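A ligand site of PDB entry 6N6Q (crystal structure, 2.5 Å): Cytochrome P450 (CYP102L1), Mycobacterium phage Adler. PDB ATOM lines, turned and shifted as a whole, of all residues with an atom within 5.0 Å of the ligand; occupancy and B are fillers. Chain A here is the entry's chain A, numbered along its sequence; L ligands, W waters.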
ATOM      1  N   LYS A  79     -15.752  20.377  -3.723  1.00  0.00           N
ATOM      2  CA  LYS A  79     -15.803  19.211  -4.590  1.00  0.00           C
ATOM      3  C   LYS A  79     -17.243  18.865  -4.964  1.00  0.00           C
ATOM      4  O   LYS A  79     -18.141  18.864  -4.116  1.00  0.00           O
ATOM      5  CB  LYS A  79     -15.147  18.002  -3.917  1.00  0.00           C
ATOM      6  CG  LYS A  79     -15.645  16.669  -4.451  1.00  0.00           C
ATOM      7  CD  LYS A  79     -14.593  15.580  -4.394  1.00  0.00           C
ATOM      8  CE  LYS A  79     -15.086  14.326  -5.108  1.00  0.00           C
ATOM      9  NZ  LYS A  79     -14.009  13.324  -5.319  1.00  0.00           N
ATOM     10  N   LEU A  85     -18.386   9.725 -10.950  1.00  0.00           N
ATOM     11  CA  LEU A  85     -18.196   9.443  -9.532  1.00  0.00           C
ATOM     12  C   LEU A  85     -19.502   8.971  -8.899  1.00  0.00           C
ATOM     13  O   LEU A  85     -19.492   8.072  -8.039  1.00  0.00           O
ATOM     14  CB  LEU A  85     -17.671  10.685  -8.803  1.00  0.00           C
ATOM     15  CG  LEU A  85     -16.162  10.898  -8.835  1.00  0.00           C
ATOM     16  CD1 LEU A  85     -15.767  12.021  -7.891  1.00  0.00           C
ATOM     17  CD2 LEU A  85     -15.439   9.614  -8.475  1.00  0.00           C
ATOM     18  N   MET A  96     -14.123   7.366   0.556  1.00  0.00           N
ATOM     19  CA  MET A  96     -13.582   8.722   0.519  1.00  0.00           C
ATOM     20  C   MET A  96     -13.642   9.328  -0.874  1.00  0.00           C
ATOM     21  O   MET A  96     -13.732  10.552  -1.008  1.00  0.00           O
ATOM     22  CB  MET A  96     -12.142   8.737   1.027  1.00  0.00           C
ATOM     23  CG  MET A  96     -12.010   8.648   2.542  1.00  0.00           C
ATOM     24  SD  MET A  96     -10.324   8.979   3.116  1.00  0.00           S
ATOM     25  CE  MET A  96     -10.060  10.619   2.457  1.00  0.00           C
ATOM     26  N   PHE A  97     -13.598   8.498  -1.922  1.00  0.00           N
ATOM     27  CA  PHE A  97     -13.519   9.030  -3.270  1.00  0.00           C
ATOM     28  C   PHE A  97     -14.899   9.369  -3.825  1.00  0.00           C
ATOM     29  O   PHE A  97     -15.058  10.357  -4.549  1.00  0.00           O
ATOM     30  CB  PHE A  97     -12.805   8.023  -4.175  1.00  0.00           C
ATOM     31  CG  PHE A  97     -12.361   8.590  -5.496  1.00  0.00           C
ATOM     32  CD1 PHE A  97     -11.644   9.773  -5.560  1.00  0.00           C
ATOM     33  CD2 PHE A  97     -12.621   7.909  -6.667  1.00  0.00           C
ATOM     34  CE1 PHE A  97     -11.226  10.293  -6.779  1.00  0.00           C
ATOM     35  CE2 PHE A  97     -12.203   8.415  -7.889  1.00  0.00           C
ATOM     36  CZ  PHE A  97     -11.505   9.603  -7.942  1.00  0.00           C
ATOM     37  N   TRP A 106     -17.481  10.759   5.050  1.00  0.00           N
ATOM     38  CA  TRP A 106     -16.311  11.345   4.417  1.00  0.00           C
ATOM     39  C   TRP A 106     -15.416  12.038   5.429  1.00  0.00           C
ATOM     40  O   TRP A 106     -14.183  11.876   5.393  1.00  0.00           O
ATOM     41  CB  TRP A 106     -16.686  12.335   3.311  1.00  0.00           C
ATOM     42  CG  TRP A 106     -15.434  13.013   2.815  1.00  0.00           C
ATOM     43  CD1 TRP A 106     -14.565  12.524   1.882  1.00  0.00           C
ATOM     44  CD2 TRP A 106     -14.877  14.237   3.294  1.00  0.00           C
ATOM     45  NE1 TRP A 106     -13.514  13.394   1.721  1.00  0.00           N
ATOM     46  CE2 TRP A 106     -13.681  14.444   2.574  1.00  0.00           C
ATOM     47  CE3 TRP A 106     -15.271  15.182   4.231  1.00  0.00           C
ATOM     48  CZ2 TRP A 106     -12.878  15.569   2.785  1.00  0.00           C
ATOM     49  CZ3 TRP A 106     -14.479  16.293   4.440  1.00  0.00           C
ATOM     50  CH2 TRP A 106     -13.293  16.481   3.710  1.00  0.00           C
ATOM     51  N   HIS A 110     -11.762  10.783   6.541  1.00  0.00           N
ATOM     52  CA  HIS A 110     -10.688  11.699   6.162  1.00  0.00           C
ATOM     53  C   HIS A 110      -9.816  12.055   7.359  1.00  0.00           C
ATOM     54  O   HIS A 110      -8.594  12.124   7.240  1.00  0.00           O
ATOM     55  CB  HIS A 110     -11.272  12.964   5.529  1.00  0.00           C
ATOM     56  CG  HIS A 110     -10.231  13.973   5.154  1.00  0.00           C
ATOM     57  ND1 HIS A 110      -9.335  13.775   4.134  1.00  0.00           N
ATOM     58  CD2 HIS A 110      -9.952  15.198   5.669  1.00  0.00           C
ATOM     59  CE1 HIS A 110      -8.537  14.824   4.027  1.00  0.00           C
ATOM     60  NE2 HIS A 110      -8.900  15.703   4.944  1.00  0.00           N
ATOM     61  N   PHE A 117      -1.286   8.327   5.499  1.00  0.00           N
ATOM     62  CA  PHE A 117      -0.855   8.722   4.168  1.00  0.00           C
ATOM     63  C   PHE A 117       0.186   9.839   4.185  1.00  0.00           C
ATOM     64  O   PHE A 117       0.481  10.411   3.134  1.00  0.00           O
ATOM     65  CB  PHE A 117      -2.063   9.163   3.322  1.00  0.00           C
ATOM     66  CG  PHE A 117      -2.881   8.025   2.802  1.00  0.00           C
ATOM     67  CD1 PHE A 117      -2.585   7.429   1.587  1.00  0.00           C
ATOM     68  CD2 PHE A 117      -3.952   7.534   3.533  1.00  0.00           C
ATOM     69  CE1 PHE A 117      -3.341   6.383   1.111  1.00  0.00           C
ATOM     70  CE2 PHE A 117      -4.709   6.488   3.056  1.00  0.00           C
ATOM     71  CZ  PHE A 117      -4.403   5.906   1.843  1.00  0.00           C
ATOM     72  N   ILE A 164      -0.472  -1.382  -3.330  1.00  0.00           N
ATOM     73  CA  ILE A 164      -1.445  -0.809  -2.393  1.00  0.00           C
ATOM     74  C   ILE A 164      -1.927  -1.882  -1.417  1.00  0.00           C
ATOM     75  O   ILE A 164      -2.017  -1.639  -0.203  1.00  0.00           O
ATOM     76  CB  ILE A 164      -2.610  -0.169  -3.152  1.00  0.00           C
ATOM     77  CG1 ILE A 164      -2.104   0.912  -4.101  1.00  0.00           C
ATOM     78  CG2 ILE A 164      -3.619   0.414  -2.172  1.00  0.00           C
ATOM     79  CD1 ILE A 164      -3.179   1.517  -4.953  1.00  0.00           C
ATOM     80  N   THR A 274     -11.993   1.470  -2.366  1.00  0.00           N
ATOM     81  CA  THR A 274     -11.617   2.792  -2.874  1.00  0.00           C
ATOM     82  C   THR A 274     -10.123   2.851  -3.176  1.00  0.00           C
ATOM     83  O   THR A 274      -9.715   3.200  -4.288  1.00  0.00           O
ATOM     84  CB  THR A 274     -11.999   3.874  -1.868  1.00  0.00           C
ATOM     85  OG1 THR A 274     -13.421   3.893  -1.703  1.00  0.00           O
ATOM     86  CG2 THR A 274     -11.509   5.232  -2.338  1.00  0.00           C
ATOM     87  N   PHE A 275      -9.286   2.509  -2.193  1.00  0.00           N
ATOM     88  CA  PHE A 275      -7.840   2.557  -2.389  1.00  0.00           C
ATOM     89  C   PHE A 275      -7.408   1.621  -3.513  1.00  0.00           C
ATOM     90  O   PHE A 275      -6.424   1.899  -4.210  1.00  0.00           O
ATOM     91  CB  PHE A 275      -7.117   2.190  -1.097  1.00  0.00           C
ATOM     92  CG  PHE A 275      -7.425   3.113   0.058  1.00  0.00           C
ATOM     93  CD1 PHE A 275      -7.998   4.363  -0.154  1.00  0.00           C
ATOM     94  CD2 PHE A 275      -7.133   2.723   1.356  1.00  0.00           C
ATOM     95  CE1 PHE A 275      -8.273   5.195   0.902  1.00  0.00           C
ATOM     96  CE2 PHE A 275      -7.417   3.559   2.422  1.00  0.00           C
ATOM     97  CZ  PHE A 275      -7.982   4.800   2.191  1.00  0.00           C
ATOM     98  N   ALA A 278      -9.123   3.546  -6.912  1.00  0.00           N
ATOM     99  CA  ALA A 278      -8.702   4.937  -7.101  1.00  0.00           C
ATOM    100  C   ALA A 278      -7.187   5.099  -7.103  1.00  0.00           C
ATOM    101  O   ALA A 278      -6.687   6.103  -7.614  1.00  0.00           O
ATOM    102  CB  ALA A 278      -9.308   5.821  -6.012  1.00  0.00           C
ATOM    103  N   GLY A 279      -6.453   4.142  -6.533  1.00  0.00           N
ATOM    104  CA  GLY A 279      -5.017   4.272  -6.437  1.00  0.00           C
ATOM    105  C   GLY A 279      -4.236   3.470  -7.463  1.00  0.00           C
ATOM    106  O   GLY A 279      -3.140   3.851  -7.857  1.00  0.00           O
ATOM    107  N   THR A 282      -4.658   4.927 -11.610  1.00  0.00           N
ATOM    108  CA  THR A 282      -3.992   6.208 -11.813  1.00  0.00           C
ATOM    109  C   THR A 282      -2.483   6.056 -11.809  1.00  0.00           C
ATOM    110  O   THR A 282      -1.795   6.548 -12.717  1.00  0.00           O
ATOM    111  CB  THR A 282      -4.431   7.204 -10.725  1.00  0.00           C
ATOM    112  OG1 THR A 282      -4.214   6.634  -9.439  1.00  0.00           O
ATOM    113  CG2 THR A 282      -5.899   7.566 -10.897  1.00  0.00           C
ATOM    114  N   SER A 283      -1.940   5.373 -10.789  1.00  0.00           N
ATOM    115  CA  SER A 283      -0.490   5.225 -10.689  1.00  0.00           C
ATOM    116  C   SER A 283       0.061   4.354 -11.805  1.00  0.00           C
ATOM    117  O   SER A 283       1.149   4.604 -12.317  1.00  0.00           O
ATOM    118  CB  SER A 283      -0.132   4.637  -9.322  1.00  0.00           C
ATOM    119  OG  SER A 283      -0.628   5.438  -8.275  1.00  0.00           O
ATOM    120  N   ALA A 286       0.166   6.328 -15.140  1.00  0.00           N
ATOM    121  CA  ALA A 286       1.217   7.341 -15.083  1.00  0.00           C
ATOM    122  C   ALA A 286       2.588   6.718 -15.306  1.00  0.00           C
ATOM    123  O   ALA A 286       3.416   7.264 -16.036  1.00  0.00           O
ATOM    124  CB  ALA A 286       1.182   8.070 -13.738  1.00  0.00           C
ATOM    125  N   LEU A 339       2.679  13.618 -15.822  1.00  0.00           N
ATOM    126  CA  LEU A 339       1.390  13.992 -15.251  1.00  0.00           C
ATOM    127  C   LEU A 339       0.886  15.314 -15.785  1.00  0.00           C
ATOM    128  O   LEU A 339      -0.310  15.612 -15.647  1.00  0.00           O
ATOM    129  CB  LEU A 339       1.488  14.037 -13.721  1.00  0.00           C
ATOM    130  CG  LEU A 339       1.597  12.674 -13.044  1.00  0.00           C
ATOM    131  CD1 LEU A 339       1.718  12.813 -11.538  1.00  0.00           C
ATOM    132  CD2 LEU A 339       0.403  11.799 -13.409  1.00  0.00           C
ATOM    133  N   VAL A 344      -3.425  11.387 -15.764  1.00  0.00           N
ATOM    134  CA  VAL A 344      -4.268  10.193 -15.752  1.00  0.00           C
ATOM    135  C   VAL A 344      -5.618  10.487 -15.127  1.00  0.00           C
ATOM    136  O   VAL A 344      -6.639   9.914 -15.529  1.00  0.00           O
ATOM    137  CB  VAL A 344      -3.538   9.033 -15.033  1.00  0.00           C
ATOM    138  CG1 VAL A 344      -2.315   8.614 -15.840  1.00  0.00           C
ATOM    139  CG2 VAL A 344      -3.128   9.440 -13.624  1.00  0.00           C
ATOM    140  N   ALA A 345      -5.663  11.383 -14.143  1.00  0.00           N
ATOM    141  CA  ALA A 345      -6.924  11.946 -13.692  1.00  0.00           C
ATOM    142  C   ALA A 345      -7.153  13.231 -14.475  1.00  0.00           C
ATOM    143  O   ALA A 345      -6.688  14.309 -14.063  1.00  0.00           O
ATOM    144  CB  ALA A 345      -6.920  12.208 -12.193  1.00  0.00           C
ATOM    145  N   TYR A 348     -11.528  17.208 -12.664  1.00  0.00           N
ATOM    146  CA  TYR A 348     -12.360  17.049 -11.489  1.00  0.00           C
ATOM    147  C   TYR A 348     -13.541  17.998 -11.578  1.00  0.00           C
ATOM    148  O   TYR A 348     -13.520  18.986 -12.318  1.00  0.00           O
ATOM    149  CB  TYR A 348     -11.563  17.301 -10.196  1.00  0.00           C
ATOM    150  CG  TYR A 348     -10.774  18.587 -10.201  1.00  0.00           C
ATOM    151  CD1 TYR A 348      -9.485  18.623 -10.717  1.00  0.00           C
ATOM    152  CD2 TYR A 348     -11.309  19.751  -9.692  1.00  0.00           C
ATOM    153  CE1 TYR A 348      -8.752  19.793 -10.728  1.00  0.00           C
ATOM    154  CE2 TYR A 348     -10.585  20.935  -9.698  1.00  0.00           C
ATOM    155  CZ  TYR A 348      -9.306  20.947 -10.211  1.00  0.00           C
ATOM    156  OH  TYR A 348      -8.582  22.118 -10.221  1.00  0.00           O
ATOM    157  N   PHE A 349     -14.586  17.681 -10.816  1.00  0.00           N
ATOM    158  CA  PHE A 349     -15.819  18.456 -10.816  1.00  0.00           C
ATOM    159  C   PHE A 349     -15.907  19.288  -9.542  1.00  0.00           C
ATOM    160  O   PHE A 349     -15.674  18.771  -8.443  1.00  0.00           O
ATOM    161  CB  PHE A 349     -17.032  17.533 -10.926  1.00  0.00           C
ATOM    162  CG  PHE A 349     -17.216  16.935 -12.284  1.00  0.00           C
ATOM    163  CD1 PHE A 349     -17.889  17.639 -13.282  1.00  0.00           C
ATOM    164  CD2 PHE A 349     -16.723  15.683 -12.582  1.00  0.00           C
ATOM    165  CE1 PHE A 349     -18.064  17.091 -14.542  1.00  0.00           C
ATOM    166  CE2 PHE A 349     -16.887  15.126 -13.838  1.00  0.00           C
ATOM    167  CZ  PHE A 349     -17.559  15.836 -14.827  1.00  0.00           C
ATOM    168  N   PRO A 411      -2.471  17.974 -10.874  1.00  0.00           N
ATOM    169  CA  PRO A 411      -2.803  16.575 -11.218  1.00  0.00           C
ATOM    170  C   PRO A 411      -3.419  15.792 -10.067  1.00  0.00           C
ATOM    171  O   PRO A 411      -3.985  14.721 -10.310  1.00  0.00           O
ATOM    172  CB  PRO A 411      -1.444  15.981 -11.624  1.00  0.00           C
ATOM    173  CG  PRO A 411      -0.446  16.814 -10.885  1.00  0.00           C
ATOM    174  CD  PRO A 411      -1.015  18.198 -10.838  1.00  0.00           C
ATOM    175  N   PHE A 412      -3.326  16.289  -8.838  1.00  0.00           N
ATOM    176  CA  PHE A 412      -3.895  15.626  -7.671  1.00  0.00           C
ATOM    177  C   PHE A 412      -5.088  16.369  -7.090  1.00  0.00           C
ATOM    178  O   PHE A 412      -5.426  16.182  -5.919  1.00  0.00           O
ATOM    179  CB  PHE A 412      -2.812  15.426  -6.597  1.00  0.00           C
ATOM    180  CG  PHE A 412      -1.686  14.538  -7.036  1.00  0.00           C
ATOM    181  CD1 PHE A 412      -1.744  13.172  -6.837  1.00  0.00           C
ATOM    182  CD2 PHE A 412      -0.550  15.085  -7.630  1.00  0.00           C
ATOM    183  CE1 PHE A 412      -0.707  12.345  -7.235  1.00  0.00           C
ATOM    184  CE2 PHE A 412       0.497  14.272  -8.026  1.00  0.00           C
ATOM    185  CZ  PHE A 412       0.418  12.900  -7.832  1.00  0.00           C
ATOM    186  N   GLY A 413      -5.734  17.222  -7.886  1.00  0.00           N
ATOM    187  CA  GLY A 413      -6.877  17.966  -7.392  1.00  0.00           C
ATOM    188  C   GLY A 413      -6.462  19.134  -6.513  1.00  0.00           C
ATOM    189  O   GLY A 413      -5.294  19.547  -6.461  1.00  0.00           O
ATOM    190  N   GLU A 416      -9.486  20.374   0.433  1.00  0.00           N
ATOM    191  CA  GLU A 416      -9.503  19.309   1.433  1.00  0.00           C
ATOM    192  C   GLU A 416      -9.798  17.949   0.814  1.00  0.00           C
ATOM    193  O   GLU A 416      -9.414  16.929   1.384  1.00  0.00           O
ATOM    194  CB  GLU A 416     -10.527  19.627   2.520  1.00  0.00           C
ATOM    195  CG  GLU A 416     -11.931  19.900   1.997  1.00  0.00           C
ATOM    196  CD  GLU A 416     -12.937  20.109   3.114  1.00  0.00           C
ATOM    197  OE1 GLU A 416     -14.132  20.312   2.804  1.00  0.00           O
ATOM    198  OE2 GLU A 416     -12.535  20.070   4.292  1.00  0.00           O
ATOM    199  N   ARG A 417     -10.467  17.913  -0.340  1.00  0.00           N
ATOM    200  CA  ARG A 417     -10.728  16.668  -1.045  1.00  0.00           C
ATOM    201  C   ARG A 417      -9.780  16.473  -2.225  1.00  0.00           C
ATOM    202  O   ARG A 417     -10.154  15.854  -3.235  1.00  0.00           O
ATOM    203  CB  ARG A 417     -12.182  16.614  -1.516  1.00  0.00           C
ATOM    204  CG  ARG A 417     -13.168  16.678  -0.370  1.00  0.00           C
ATOM    205  CD  ARG A 417     -14.492  16.044  -0.719  1.00  0.00           C
ATOM    206  NE  ARG A 417     -14.359  14.622  -1.056  1.00  0.00           N
ATOM    207  CZ  ARG A 417     -15.382  13.818  -1.315  1.00  0.00           C
ATOM    208  NH1 ARG A 417     -16.619  14.293  -1.284  1.00  0.00           N
ATOM    209  NH2 ARG A 417     -15.171  12.541  -1.620  1.00  0.00           N
ATOM    210  N   ALA A 418      -8.561  16.992  -2.126  1.00  0.00           N
ATOM    211  CA  ALA A 418      -7.504  16.604  -3.044  1.00  0.00           C
ATOM    212  C   ALA A 418      -7.050  15.186  -2.717  1.00  0.00           C
ATOM    213  O   ALA A 418      -7.516  14.556  -1.768  1.00  0.00           O
ATOM    214  CB  ALA A 418      -6.341  17.597  -2.984  1.00  0.00           C
ATOM    215  N   CYS A 419      -6.114  14.672  -3.511  1.00  0.00           N
ATOM    216  CA  CYS A 419      -5.729  13.266  -3.422  1.00  0.00           C
ATOM    217  C   CYS A 419      -5.036  12.977  -2.093  1.00  0.00           C
ATOM    218  O   CYS A 419      -3.939  13.483  -1.833  1.00  0.00           O
ATOM    219  CB  CYS A 419      -4.821  12.883  -4.576  1.00  0.00           C
ATOM    220  SG  CYS A 419      -4.218  11.195  -4.451  1.00  0.00           S
ATOM    221  N   ILE A 420      -5.657  12.126  -1.264  1.00  0.00           N
ATOM    222  CA  ILE A 420      -5.038  11.723  -0.012  1.00  0.00           C
ATOM    223  C   ILE A 420      -3.808  10.853  -0.247  1.00  0.00           C
ATOM    224  O   ILE A 420      -2.953  10.746   0.636  1.00  0.00           O
ATOM    225  CB  ILE A 420      -6.049  10.996   0.882  1.00  0.00           C
ATOM    226  CG1 ILE A 420      -5.554  10.944   2.330  1.00  0.00           C
ATOM    227  CG2 ILE A 420      -6.300   9.588   0.370  1.00  0.00           C
ATOM    228  CD1 ILE A 420      -6.468  10.172   3.266  1.00  0.00           C
ATOM    229  N   GLY A 421      -3.679  10.246  -1.428  1.00  0.00           N
ATOM    230  CA  GLY A 421      -2.572   9.344  -1.692  1.00  0.00           C
ATOM    231  C   GLY A 421      -1.505   9.929  -2.597  1.00  0.00           C
ATOM    232  O   GLY A 421      -0.809   9.185  -3.298  1.00  0.00           O
ATOM    233  N   PHE A 424       1.859   8.859  -1.396  1.00  0.00           N
ATOM    234  CA  PHE A 424       1.980   7.428  -1.667  1.00  0.00           C
ATOM    235  C   PHE A 424       2.259   7.187  -3.146  1.00  0.00           C
ATOM    236  O   PHE A 424       3.130   6.382  -3.496  1.00  0.00           O
ATOM    237  CB  PHE A 424       0.702   6.708  -1.236  1.00  0.00           C
ATOM    238  CG  PHE A 424       0.802   5.199  -1.282  1.00  0.00           C
ATOM    239  CD1 PHE A 424       0.591   4.510  -2.476  1.00  0.00           C
ATOM    240  CD2 PHE A 424       1.099   4.477  -0.145  1.00  0.00           C
ATOM    241  CE1 PHE A 424       0.686   3.132  -2.519  1.00  0.00           C
ATOM    242  CE2 PHE A 424       1.195   3.099  -0.188  1.00  0.00           C
ATOM    243  CZ  PHE A 424       0.983   2.424  -1.379  1.00  0.00           C
ATOM    244  N   ALA A 425       1.531   7.876  -4.023  1.00  0.00           N
ATOM    245  CA  ALA A 425       1.702   7.681  -5.463  1.00  0.00           C
ATOM    246  C   ALA A 425       3.091   8.137  -5.905  1.00  0.00           C
ATOM    247  O   ALA A 425       3.769   7.428  -6.661  1.00  0.00           O
ATOM    248  CB  ALA A 425       0.612   8.418  -6.230  1.00  0.00           C
ATOM    249  N   GLU A 428       5.752   5.509  -4.834  1.00  0.00           N
ATOM    250  CA  GLU A 428       5.759   4.249  -5.578  1.00  0.00           C
ATOM    251  C   GLU A 428       6.122   4.449  -7.042  1.00  0.00           C
ATOM    252  O   GLU A 428       6.712   3.562  -7.668  1.00  0.00           O
ATOM    253  CB  GLU A 428       4.412   3.547  -5.470  1.00  0.00           C
ATOM    254  CG  GLU A 428       3.248   4.311  -6.083  1.00  0.00           C
ATOM    255  CD  GLU A 428       2.029   3.445  -6.310  1.00  0.00           C
ATOM    256  OE1 GLU A 428       2.197   2.293  -6.770  1.00  0.00           O
ATOM    257  OE2 GLU A 428       0.903   3.921  -6.029  1.00  0.00           O
ATOM    258  N   MET A 429       5.792   5.616  -7.613  1.00  0.00           N
ATOM    259  CA  MET A 429       6.099   5.853  -9.025  1.00  0.00           C
ATOM    260  C   MET A 429       7.597   6.018  -9.251  1.00  0.00           C
ATOM    261  O   MET A 429       8.106   5.604 -10.303  1.00  0.00           O
ATOM    262  CB  MET A 429       5.341   7.083  -9.526  1.00  0.00           C
ATOM    263  CG  MET A 429       3.847   6.872  -9.707  1.00  0.00           C
ATOM    264  SD  MET A 429       3.009   8.269 -10.480  1.00  0.00           S
ATOM    265  CE  MET A 429       3.277   9.560  -9.274  1.00  0.00           C
HETATM  266  C1  LIG L   1      -8.499  11.883  -4.944  1.00  0.00           C
HETATM  267  C2  LIG L   1      -5.455  11.798  -8.727  1.00  0.00           C
HETATM  268  C3  LIG L   1      -3.068   8.065  -6.714  1.00  0.00           C
HETATM  269  C4  LIG L   1      -6.557   7.700  -3.356  1.00  0.00           C
HETATM  270  C5  LIG L   1      -7.878  12.210  -6.133  1.00  0.00           C
HETATM  271  C6  LIG L   1      -8.211  13.320  -7.011  1.00  0.00           C
HETATM  272  C7  LIG L   1      -7.375  13.293  -8.048  1.00  0.00           C
HETATM  273  C8  LIG L   1      -6.469  12.173  -7.877  1.00  0.00           C
HETATM  274  C9  LIG L   1      -7.367  14.292  -9.231  1.00  0.00           C
HETATM  275  C10 LIG L   1      -9.340  14.351  -6.801  1.00  0.00           C
HETATM  276  C11 LIG L   1     -10.634  13.780  -7.380  1.00  0.00           C
HETATM  277  C12 LIG L   1     -11.726  14.823  -7.370  1.00  0.00           C
HETATM  278  O1  LIG L   1     -11.445  16.003  -7.027  1.00  0.00           O
HETATM  279  O2  LIG L   1     -12.888  14.470  -7.694  1.00  0.00           O
HETATM  280  C13 LIG L   1      -4.506  10.822  -8.483  1.00  0.00           C
HETATM  281  C14 LIG L   1      -3.309  10.574  -9.276  1.00  0.00           C
HETATM  282  C15 LIG L   1      -2.644   9.540  -8.723  1.00  0.00           C
HETATM  283  C16 LIG L   1      -3.405   9.096  -7.566  1.00  0.00           C
HETATM  284  C17 LIG L   1      -2.938  11.412 -10.521  1.00  0.00           C
HETATM  285  C18 LIG L   1      -1.315   8.871  -9.150  1.00  0.00           C
HETATM  286  C19 LIG L   1      -0.590   9.208 -10.225  1.00  0.00           C
HETATM  287  C20 LIG L   1      -3.776   7.641  -5.611  1.00  0.00           C
HETATM  288  C21 LIG L   1      -3.388   6.611  -4.670  1.00  0.00           C
HETATM  289  C22 LIG L   1      -4.343   6.497  -3.746  1.00  0.00           C
HETATM  290  C23 LIG L   1      -5.389   7.472  -4.052  1.00  0.00           C
HETATM  291  C24 LIG L   1      -2.098   5.764  -4.724  1.00  0.00           C
HETATM  292  C25 LIG L   1      -4.261   5.487  -2.577  1.00  0.00           C
HETATM  293  C26 LIG L   1      -5.204   5.403  -1.627  1.00  0.00           C
HETATM  294  C27 LIG L   1      -7.386   8.810  -3.481  1.00  0.00           C
HETATM  295  C28 LIG L   1      -8.541   9.108  -2.652  1.00  0.00           C
HETATM  296  C29 LIG L   1      -9.076  10.261  -3.091  1.00  0.00           C
HETATM  297  C30 LIG L   1      -8.281  10.733  -4.208  1.00  0.00           C
HETATM  298  C31 LIG L   1      -9.070   8.255  -1.477  1.00  0.00           C
HETATM  299  C32 LIG L   1     -10.318  10.966  -2.505  1.00  0.00           C
HETATM  300  C33 LIG L   1      -9.913  11.827  -1.317  1.00  0.00           C
HETATM  301  C34 LIG L   1     -11.116  12.595  -0.809  1.00  0.00           C
HETATM  302  O3  LIG L   1     -11.165  12.878   0.423  1.00  0.00           O
HETATM  303  O4  LIG L   1     -12.022  12.916  -1.619  1.00  0.00           O
HETATM  304  N1  LIG L   1      -6.817  11.541  -6.701  1.00  0.00           N
HETATM  305  N2  LIG L   1      -4.526   9.903  -7.455  1.00  0.00           N
HETATM  306  N3  LIG L   1      -4.999   8.140  -5.194  1.00  0.00           N
HETATM  307  N4  LIG L   1      -7.259   9.818  -4.420  1.00  0.00           N
HETATM  308 FE1  LIG L   1      -5.973   9.759  -6.021  1.00  0.00          FE
HETATM  309  O   HOH W   1     -14.868  15.610  -9.101  1.00  0.00           O
HETATM  310  O   HOH W   2     -13.236  18.006  -7.027  1.00  0.00           O
HETATM  311  O   HOH W   3      -9.696  17.533  -5.903  1.00  0.00           O
HETATM  312  O   HOH W   4     -11.788  13.557  -4.097  1.00  0.00           O
HETATM  313  O   HOH W   5     -12.665  12.973 -10.032  1.00  0.00           O
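Residues that only touch the ligand: Leu 85 (3.8 Å), Phe 97 (3.5 Å), Phe 117 (3.5 Å), Thr 274 (3.98 Å), Phe 275 (3.3 Å), Ala 278 (3.6 Å), Gly 279 (3.4 Å), Thr 282 (3.2 Å), Ser 283 (3.6 Å), Val 344 (3.7 Å), Ala 345 (3.6 Å), Tyr 348 (3.4 Å), Pro 411 (3.5 Å), Phe 412 (3.7 Å), Gly 413 (3.6 Å), Ala 418 (3.7 Å), Ile 420 (3.6 Å), Gly 421 (3.9 Å), Phe 424 (3.7 Å), Ala 425 (3.5 Å), Glu 428 (3.8 Å) and Met 429 (3.7 Å).
Hydrophobic or aromatic side chains within 4 Å of the ligand: Leu 85, Met 96, Phe 97, Trp 106, Phe 117, Phe 275, Val 344, Ala 345, Tyr 348, Phe 412, Ile 420, Phe 424, Ala 425 and Met 429.
27 residues have an atom within 4 Å of the ligand: Lys 79, Leu 85, Met 96, Phe 97, Trp 106, Phe 117, Thr 274, Phe 275, Ala 278, Gly 279, Thr 282, Ser 283, Val 344, Ala 345, Tyr 348, Pro 411, Phe 412, Gly 413, Arg 417, Ala 418, Cys 419, Ile 420, Gly 421, Phe 424, Ala 425, Glu 428 and Met 429.
The nearest printed residue that does not touch the ligand is Ala 286 (4.1 Å).
The side-chain hydroxyl (OG) of Ser 283 is in hydrogen-bond range of the side-chain carboxylate (OE2) of Glu 428 (3.1 Å).
The side-chain hydroxyl (OG1) of Thr 282 is in hydrogen-bond range of the backbone carbonyl oxygen (O) of Ala 278 (3.1 Å).
O of Gly 279 lies within hydrogen-bond range of OG of Ser 283.
The backbone carbonyl oxygen (O) of Phe 97 sits at hydrogen-bond distance from the side-chain amino group (NZ) of Lys 79, 3.2 Å away.
The backbone NH (N) of Gly 421 lies close to the side-chain sulfur (SG) of Cys 419.
OG1 of Thr 282 sits at hydrogen-bond distance from O of Gly 279.
The backbone carbonyl oxygen (O) of Phe 412 sits at hydrogen-bond distance from the backbone NH (N) of Cys 419.
The guanidinium group of Arg 417 is in hydrogen-bond range of the backbone carbonyl oxygen of Met 96.
An iron atom (FE1) of the ligand is bound by the side-chain sulfur of Cys 419, 2.8 Å away.
An oxygen (O3) of the ligand is in hydrogen-bond range of the indole nitrogen of Trp 106 (2.7 Å).
O4 of the ligand lies within salt-bridge range of NE of Arg 417.
The backbone carbonyl oxygen (O) of Met 96 lies close to an oxygen (O4) of the ligand, 3.0 Å away.
O2 of the ligand is in salt-bridge range of NZ of Lys 79, at 2.9 Å.
Water W4 lies within hydrogen-bond range of NZ of Lys 79 (2.5 Å), O4 of the ligand (2.6 Å) and O of Arg 417 (2.9 Å).
Water W3 lies within hydrogen-bond range of an oxygen (O1) of the ligand (2.6 Å) and the backbone carbonyl oxygen of Arg 417 (3.2 Å).
Water W1 lies within hydrogen-bond range of O2 of the ligand (2.7 Å) and N of Phe 349 (2.7 Å).
Water W2 lies within hydrogen-bond range of an oxygen (O1) of the ligand (2.7 Å) and the backbone carbonyl oxygen (O) of Phe 349 (2.9 Å).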
